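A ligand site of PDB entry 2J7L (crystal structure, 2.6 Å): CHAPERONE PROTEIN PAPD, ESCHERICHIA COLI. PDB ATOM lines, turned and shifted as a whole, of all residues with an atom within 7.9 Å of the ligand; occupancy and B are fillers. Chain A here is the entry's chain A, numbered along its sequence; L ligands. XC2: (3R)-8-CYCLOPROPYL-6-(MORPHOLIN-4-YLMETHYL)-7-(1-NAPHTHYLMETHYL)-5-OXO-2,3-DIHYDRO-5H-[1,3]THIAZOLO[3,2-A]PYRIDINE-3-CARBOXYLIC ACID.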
ATOM      1  N   PRO A  30      18.830 -17.912  22.278  1.00  0.00           N
ATOM      2  CA  PRO A  30      18.841 -18.639  21.015  1.00  0.00           C
ATOM      3  C   PRO A  30      20.117 -18.352  20.206  1.00  0.00           C
ATOM      4  O   PRO A  30      20.582 -17.204  20.127  1.00  0.00           O
ATOM      5  CB  PRO A  30      17.587 -18.116  20.336  1.00  0.00           C
ATOM      6  CG  PRO A  30      17.606 -16.673  20.722  1.00  0.00           C
ATOM      7  CD  PRO A  30      17.939 -16.748  22.204  1.00  0.00           C
ATOM      8  N   TYR A  31      20.686 -19.389  19.587  1.00  0.00           N
ATOM      9  CA  TYR A  31      21.899 -19.235  18.781  1.00  0.00           C
ATOM     10  C   TYR A  31      21.725 -19.835  17.390  1.00  0.00           C
ATOM     11  O   TYR A  31      20.813 -20.622  17.141  1.00  0.00           O
ATOM     12  CB  TYR A  31      23.089 -19.926  19.468  1.00  0.00           C
ATOM     13  CG  TYR A  31      23.859 -19.092  20.470  1.00  0.00           C
ATOM     14  CD1 TYR A  31      23.345 -18.796  21.737  1.00  0.00           C
ATOM     15  CD2 TYR A  31      25.132 -18.592  20.153  1.00  0.00           C
ATOM     16  CE1 TYR A  31      24.062 -18.025  22.662  1.00  0.00           C
ATOM     17  CE2 TYR A  31      25.851 -17.826  21.062  1.00  0.00           C
ATOM     18  CZ  TYR A  31      25.328 -17.542  22.313  1.00  0.00           C
ATOM     19  OH  TYR A  31      26.057 -16.777  23.199  1.00  0.00           O
ATOM     20  N   LEU A  32      22.605 -19.455  16.466  1.00  0.00           N
ATOM     21  CA  LEU A  32      22.566 -20.015  15.120  1.00  0.00           C
ATOM     22  C   LEU A  32      23.757 -20.977  14.954  1.00  0.00           C
ATOM     23  O   LEU A  32      24.834 -20.728  15.485  1.00  0.00           O
ATOM     24  CB  LEU A  32      22.621 -18.912  14.061  1.00  0.00           C
ATOM     25  CG  LEU A  32      21.442 -17.937  14.018  1.00  0.00           C
ATOM     26  CD1 LEU A  32      21.621 -17.024  12.821  1.00  0.00           C
ATOM     27  CD2 LEU A  32      20.105 -18.678  13.914  1.00  0.00           C
ATOM     28  N   ALA A  33      23.541 -22.077  14.244  1.00  0.00           N
ATOM     29  CA  ALA A  33      24.584 -23.066  14.001  1.00  0.00           C
ATOM     30  C   ALA A  33      24.928 -23.074  12.533  1.00  0.00           C
ATOM     31  O   ALA A  33      24.132 -23.494  11.685  1.00  0.00           O
ATOM     32  CB  ALA A  33      24.124 -24.460  14.429  1.00  0.00           C
ATOM     33  N   GLN A  34      26.124 -22.612  12.226  1.00  0.00           N
ATOM     34  CA  GLN A  34      26.560 -22.577  10.857  1.00  0.00           C
ATOM     35  C   GLN A  34      27.577 -23.698  10.636  1.00  0.00           C
ATOM     36  O   GLN A  34      28.514 -23.865  11.422  1.00  0.00           O
ATOM     37  CB  GLN A  34      27.163 -21.238  10.596  1.00  0.00           C
ATOM     38  CG  GLN A  34      27.544 -21.028   9.191  1.00  0.00           C
ATOM     39  CD  GLN A  34      27.932 -19.602   8.991  1.00  0.00           C
ATOM     40  OE1 GLN A  34      28.757 -19.065   9.748  1.00  0.00           O
ATOM     41  NE2 GLN A  34      27.328 -18.951   7.991  1.00  0.00           N
ATOM     42  N   PRO A  55      23.272 -25.367   5.926  1.00  0.00           N
ATOM     43  CA  PRO A  55      24.412 -24.484   6.176  1.00  0.00           C
ATOM     44  C   PRO A  55      24.202 -23.682   7.447  1.00  0.00           C
ATOM     45  O   PRO A  55      25.110 -23.519   8.266  1.00  0.00           O
ATOM     46  CB  PRO A  55      24.481 -23.629   4.914  1.00  0.00           C
ATOM     47  CG  PRO A  55      23.075 -23.623   4.425  1.00  0.00           C
ATOM     48  CD  PRO A  55      22.609 -25.037   4.653  1.00  0.00           C
ATOM     49  N   VAL A  56      22.973 -23.197   7.630  1.00  0.00           N
ATOM     50  CA  VAL A  56      22.634 -22.408   8.803  1.00  0.00           C
ATOM     51  C   VAL A  56      21.299 -22.878   9.327  1.00  0.00           C
ATOM     52  O   VAL A  56      20.415 -23.233   8.550  1.00  0.00           O
ATOM     53  CB  VAL A  56      22.528 -20.923   8.436  1.00  0.00           C
ATOM     54  CG1 VAL A  56      22.472 -20.082   9.706  1.00  0.00           C
ATOM     55  CG2 VAL A  56      23.699 -20.518   7.551  1.00  0.00           C
ATOM     56  N   GLN A  57      21.162 -22.881  10.642  1.00  0.00           N
ATOM     57  CA  GLN A  57      19.919 -23.290  11.276  1.00  0.00           C
ATOM     58  C   GLN A  57      19.871 -22.629  12.642  1.00  0.00           C
ATOM     59  O   GLN A  57      20.901 -22.301  13.216  1.00  0.00           O
ATOM     60  CB  GLN A  57      19.847 -24.809  11.443  1.00  0.00           C
ATOM     61  CG  GLN A  57      20.946 -25.385  12.307  1.00  0.00           C
ATOM     62  CD  GLN A  57      20.764 -26.858  12.541  1.00  0.00           C
ATOM     63  OE1 GLN A  57      19.830 -27.284  13.233  1.00  0.00           O
ATOM     64  NE2 GLN A  57      21.646 -27.666  11.957  1.00  0.00           N
ATOM     65  N   ARG A  58      18.656 -22.428  13.160  1.00  0.00           N
ATOM     66  CA  ARG A  58      18.506 -21.807  14.450  1.00  0.00           C
ATOM     67  C   ARG A  58      18.193 -22.841  15.519  1.00  0.00           C
ATOM     68  O   ARG A  58      17.489 -23.827  15.278  1.00  0.00           O
ATOM     69  CB  ARG A  58      17.391 -20.751  14.386  1.00  0.00           C
ATOM     70  CG  ARG A  58      16.999 -20.168  15.734  1.00  0.00           C
ATOM     71  CD  ARG A  58      15.991 -19.034  15.608  1.00  0.00           C
ATOM     72  NE  ARG A  58      15.358 -18.770  16.912  1.00  0.00           N
ATOM     73  CZ  ARG A  58      15.137 -17.562  17.418  1.00  0.00           C
ATOM     74  NH1 ARG A  58      15.487 -16.464  16.747  1.00  0.00           N
ATOM     75  NH2 ARG A  58      14.559 -17.460  18.616  1.00  0.00           N
ATOM     76  N   LEU A  59      18.755 -22.607  16.709  1.00  0.00           N
ATOM     77  CA  LEU A  59      18.543 -23.479  17.859  1.00  0.00           C
ATOM     78  C   LEU A  59      18.107 -22.652  19.061  1.00  0.00           C
ATOM     79  O   LEU A  59      18.889 -21.868  19.615  1.00  0.00           O
ATOM     80  CB  LEU A  59      19.825 -24.266  18.200  1.00  0.00           C
ATOM     81  CG  LEU A  59      20.241 -25.473  17.341  1.00  0.00           C
ATOM     82  CD1 LEU A  59      20.615 -25.028  15.938  1.00  0.00           C
ATOM     83  CD2 LEU A  59      21.418 -26.167  18.014  1.00  0.00           C
ATOM     84  N   ASP A  60      16.853 -22.810  19.448  1.00  0.00           N
ATOM     85  CA  ASP A  60      16.330 -22.076  20.583  1.00  0.00           C
ATOM     86  C   ASP A  60      17.004 -22.585  21.866  1.00  0.00           C
ATOM     87  O   ASP A  60      17.536 -23.692  21.894  1.00  0.00           O
ATOM     88  CB  ASP A  60      14.803 -22.234  20.645  1.00  0.00           C
ATOM     89  CG  ASP A  60      14.097 -21.455  19.534  1.00  0.00           C
ATOM     90  OD1 ASP A  60      12.944 -21.795  19.220  1.00  0.00           O
ATOM     91  OD2 ASP A  60      14.674 -20.488  18.994  1.00  0.00           O
ATOM     92  N   ILE A  93      26.238 -18.234  16.050  1.00  0.00           N
ATOM     93  CA  ILE A  93      25.847 -16.829  15.914  1.00  0.00           C
ATOM     94  C   ILE A  93      24.856 -16.513  17.018  1.00  0.00           C
ATOM     95  O   ILE A  93      23.708 -16.979  16.987  1.00  0.00           O
ATOM     96  CB  ILE A  93      25.190 -16.555  14.562  1.00  0.00           C
ATOM     97  CG1 ILE A  93      26.130 -16.996  13.447  1.00  0.00           C
ATOM     98  CG2 ILE A  93      24.910 -15.069  14.402  1.00  0.00           C
ATOM     99  CD1 ILE A  93      25.549 -16.800  12.095  1.00  0.00           C
ATOM    100  N   PRO A  94      25.287 -15.721  18.001  1.00  0.00           N
ATOM    101  CA  PRO A  94      24.491 -15.293  19.163  1.00  0.00           C
ATOM    102  C   PRO A  94      23.326 -14.368  18.810  1.00  0.00           C
ATOM    103  O   PRO A  94      23.131 -14.015  17.645  1.00  0.00           O
ATOM    104  CB  PRO A  94      25.522 -14.607  20.028  1.00  0.00           C
ATOM    105  CG  PRO A  94      26.353 -13.904  18.991  1.00  0.00           C
ATOM    106  CD  PRO A  94      26.574 -14.993  17.975  1.00  0.00           C
ATOM    107  N   PRO A  95      22.514 -13.975  19.812  1.00  0.00           N
ATOM    108  CA  PRO A  95      21.404 -13.075  19.523  1.00  0.00           C
ATOM    109  C   PRO A  95      21.944 -11.744  19.003  1.00  0.00           C
ATOM    110  O   PRO A  95      22.958 -11.253  19.491  1.00  0.00           O
ATOM    111  CB  PRO A  95      20.718 -12.938  20.873  1.00  0.00           C
ATOM    112  CG  PRO A  95      20.921 -14.301  21.473  1.00  0.00           C
ATOM    113  CD  PRO A  95      22.374 -14.567  21.160  1.00  0.00           C
ATOM    114  N   ARG A  96      21.270 -11.162  18.013  1.00  0.00           N
ATOM    115  CA  ARG A  96      21.757  -9.914  17.448  1.00  0.00           C
ATOM    116  C   ARG A  96      21.761  -8.736  18.442  1.00  0.00           C
ATOM    117  O   ARG A  96      21.980  -7.586  18.081  1.00  0.00           O
ATOM    118  CB  ARG A  96      20.972  -9.570  16.163  1.00  0.00           C
ATOM    119  CG  ARG A  96      19.486  -9.336  16.319  1.00  0.00           C
ATOM    120  CD  ARG A  96      18.858  -9.088  14.945  1.00  0.00           C
ATOM    121  NE  ARG A  96      17.650  -8.284  15.032  1.00  0.00           N
ATOM    122  CZ  ARG A  96      16.484  -8.712  15.527  1.00  0.00           C
ATOM    123  NH1 ARG A  96      16.361  -9.945  15.994  1.00  0.00           N
ATOM    124  NH2 ARG A  96      15.443  -7.877  15.575  1.00  0.00           N
ATOM    125  N   SER A  97      21.539  -9.073  19.708  1.00  0.00           N
ATOM    126  CA  SER A  97      21.547  -8.099  20.794  1.00  0.00           C
ATOM    127  C   SER A  97      22.975  -7.578  20.952  1.00  0.00           C
ATOM    128  O   SER A  97      23.213  -6.530  21.554  1.00  0.00           O
ATOM    129  CB  SER A  97      21.082  -8.775  22.091  1.00  0.00           C
ATOM    130  OG  SER A  97      19.919  -9.560  21.857  1.00  0.00           O
ATOM    131  N   GLU A  98      23.936  -8.324  20.405  1.00  0.00           N
ATOM    132  CA  GLU A  98      25.350  -7.967  20.468  1.00  0.00           C
ATOM    133  C   GLU A  98      25.761  -7.116  19.273  1.00  0.00           C
ATOM    134  O   GLU A  98      26.920  -7.123  18.868  1.00  0.00           O
ATOM    135  CB  GLU A  98      26.223  -9.223  20.509  1.00  0.00           C
ATOM    136  CG  GLU A  98      26.453  -9.809  21.894  1.00  0.00           C
ATOM    137  CD  GLU A  98      25.189 -10.393  22.511  1.00  0.00           C
ATOM    138  OE1 GLU A  98      25.263 -10.840  23.684  1.00  0.00           O
ATOM    139  OE2 GLU A  98      24.138 -10.412  21.843  1.00  0.00           O
HETATM  140  S6  XC2 L   1      21.113 -12.757  13.663  1.00  0.00           S
HETATM  141  C5  XC2 L   1      21.062 -13.871  15.083  1.00  0.00           C
HETATM  142  C11 XC2 L   1      19.564 -14.218  15.224  1.00  0.00           C
HETATM  143  N10 XC2 L   1      19.041 -14.316  13.845  1.00  0.00           N
HETATM  144  C6  XC2 L   1      19.716 -13.627  12.930  1.00  0.00           C
HETATM  145  C7  XC2 L   1      19.364 -13.593  11.615  1.00  0.00           C
HETATM  146  C8  XC2 L   1      18.152 -14.423  11.199  1.00  0.00           C
HETATM  147  C9  XC2 L   1      17.472 -15.139  12.166  1.00  0.00           C
HETATM  148  C10 XC2 L   1      17.981 -15.066  13.576  1.00  0.00           C
HETATM  149  O25 XC2 L   1      17.375 -15.695  14.428  1.00  0.00           O
HETATM  150  C26 XC2 L   1      16.248 -15.988  11.849  1.00  0.00           C
HETATM  151  N5  XC2 L   1      16.638 -17.178  11.053  1.00  0.00           N
HETATM  152  C1  XC2 L   1      15.460 -17.636  10.270  1.00  0.00           C
HETATM  153  C2  XC2 L   1      15.858 -18.892   9.438  1.00  0.00           C
HETATM  154  O3  XC2 L   1      16.367 -19.931  10.311  1.00  0.00           O
HETATM  155  C34 XC2 L   1      17.521 -19.500  11.068  1.00  0.00           C
HETATM  156  C4  XC2 L   1      17.119 -18.261  11.962  1.00  0.00           C
HETATM  157  C24 XC2 L   1      17.684 -14.428   9.737  1.00  0.00           C
HETATM  158  C15 XC2 L   1      18.397 -15.496   8.834  1.00  0.00           C
HETATM  159  C20 XC2 L   1      19.516 -16.250   9.322  1.00  0.00           C
HETATM  160  C19 XC2 L   1      20.167 -17.211   8.513  1.00  0.00           C
HETATM  161  C18 XC2 L   1      19.715 -17.450   7.192  1.00  0.00           C
HETATM  162  C17 XC2 L   1      18.591 -16.735   6.673  1.00  0.00           C
HETATM  163  C21 XC2 L   1      18.140 -16.994   5.341  1.00  0.00           C
HETATM  164  C27 XC2 L   1      17.023 -16.275   4.815  1.00  0.00           C
HETATM  165  C28 XC2 L   1      16.360 -15.303   5.606  1.00  0.00           C
HETATM  166  C29 XC2 L   1      16.800 -15.037   6.933  1.00  0.00           C
HETATM  167  C16 XC2 L   1      17.928 -15.748   7.489  1.00  0.00           C
HETATM  168  C22 XC2 L   1      20.065 -12.836  10.482  1.00  0.00           C
HETATM  169  C31 XC2 L   1      19.820 -11.302  10.599  1.00  0.00           C
HETATM  170  C30 XC2 L   1      21.268 -11.919  10.540  1.00  0.00           C
HETATM  171  C23 XC2 L   1      18.833 -13.079  15.991  1.00  0.00           C
HETATM  172  O33 XC2 L   1      19.195 -12.891  17.255  1.00  0.00           O
HETATM  173  O32 XC2 L   1      17.961 -12.402  15.463  1.00  0.00           O
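The backbone NH of Arg 96 sits at hydrogen-bond distance from an oxygen (O33) of the ligand, 2.8 Å away.
NH1 of Arg 96 is in salt-bridge range of O32 of the ligand (3.0 Å).
An oxygen (O25) of the ligand lies within hydrogen-bond range of the guanidinium group (NH1) of Arg 58 (3.1 Å).
The guanidinium group of Arg 58 is in salt-bridge range of the side-chain carboxylate of Asp 60, at 2.8 Å.
N of Leu 32 is in hydrogen-bond range of O of Ile 93, at 2.8 Å.
Leu 32 touches the ligand (CD2 to C4, 3.6 Å).
Val 56 touches the ligand (CG1 to C19, 3.9 Å).
O of Pro 94 touches C5 of the ligand (3.3 Å).
Pro 95 touches the ligand (CA to O33, 3.2 Å).
Within 4 Å of the ligand: Leu 32, Val 56, Arg 58, Pro 94, Pro 95 and Arg 96.
Along chain A the residues within 4 Å of the ligand span positions 32 to 96.
The nearest printed residue that does not touch the ligand is Ile 93 (4.1 Å).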
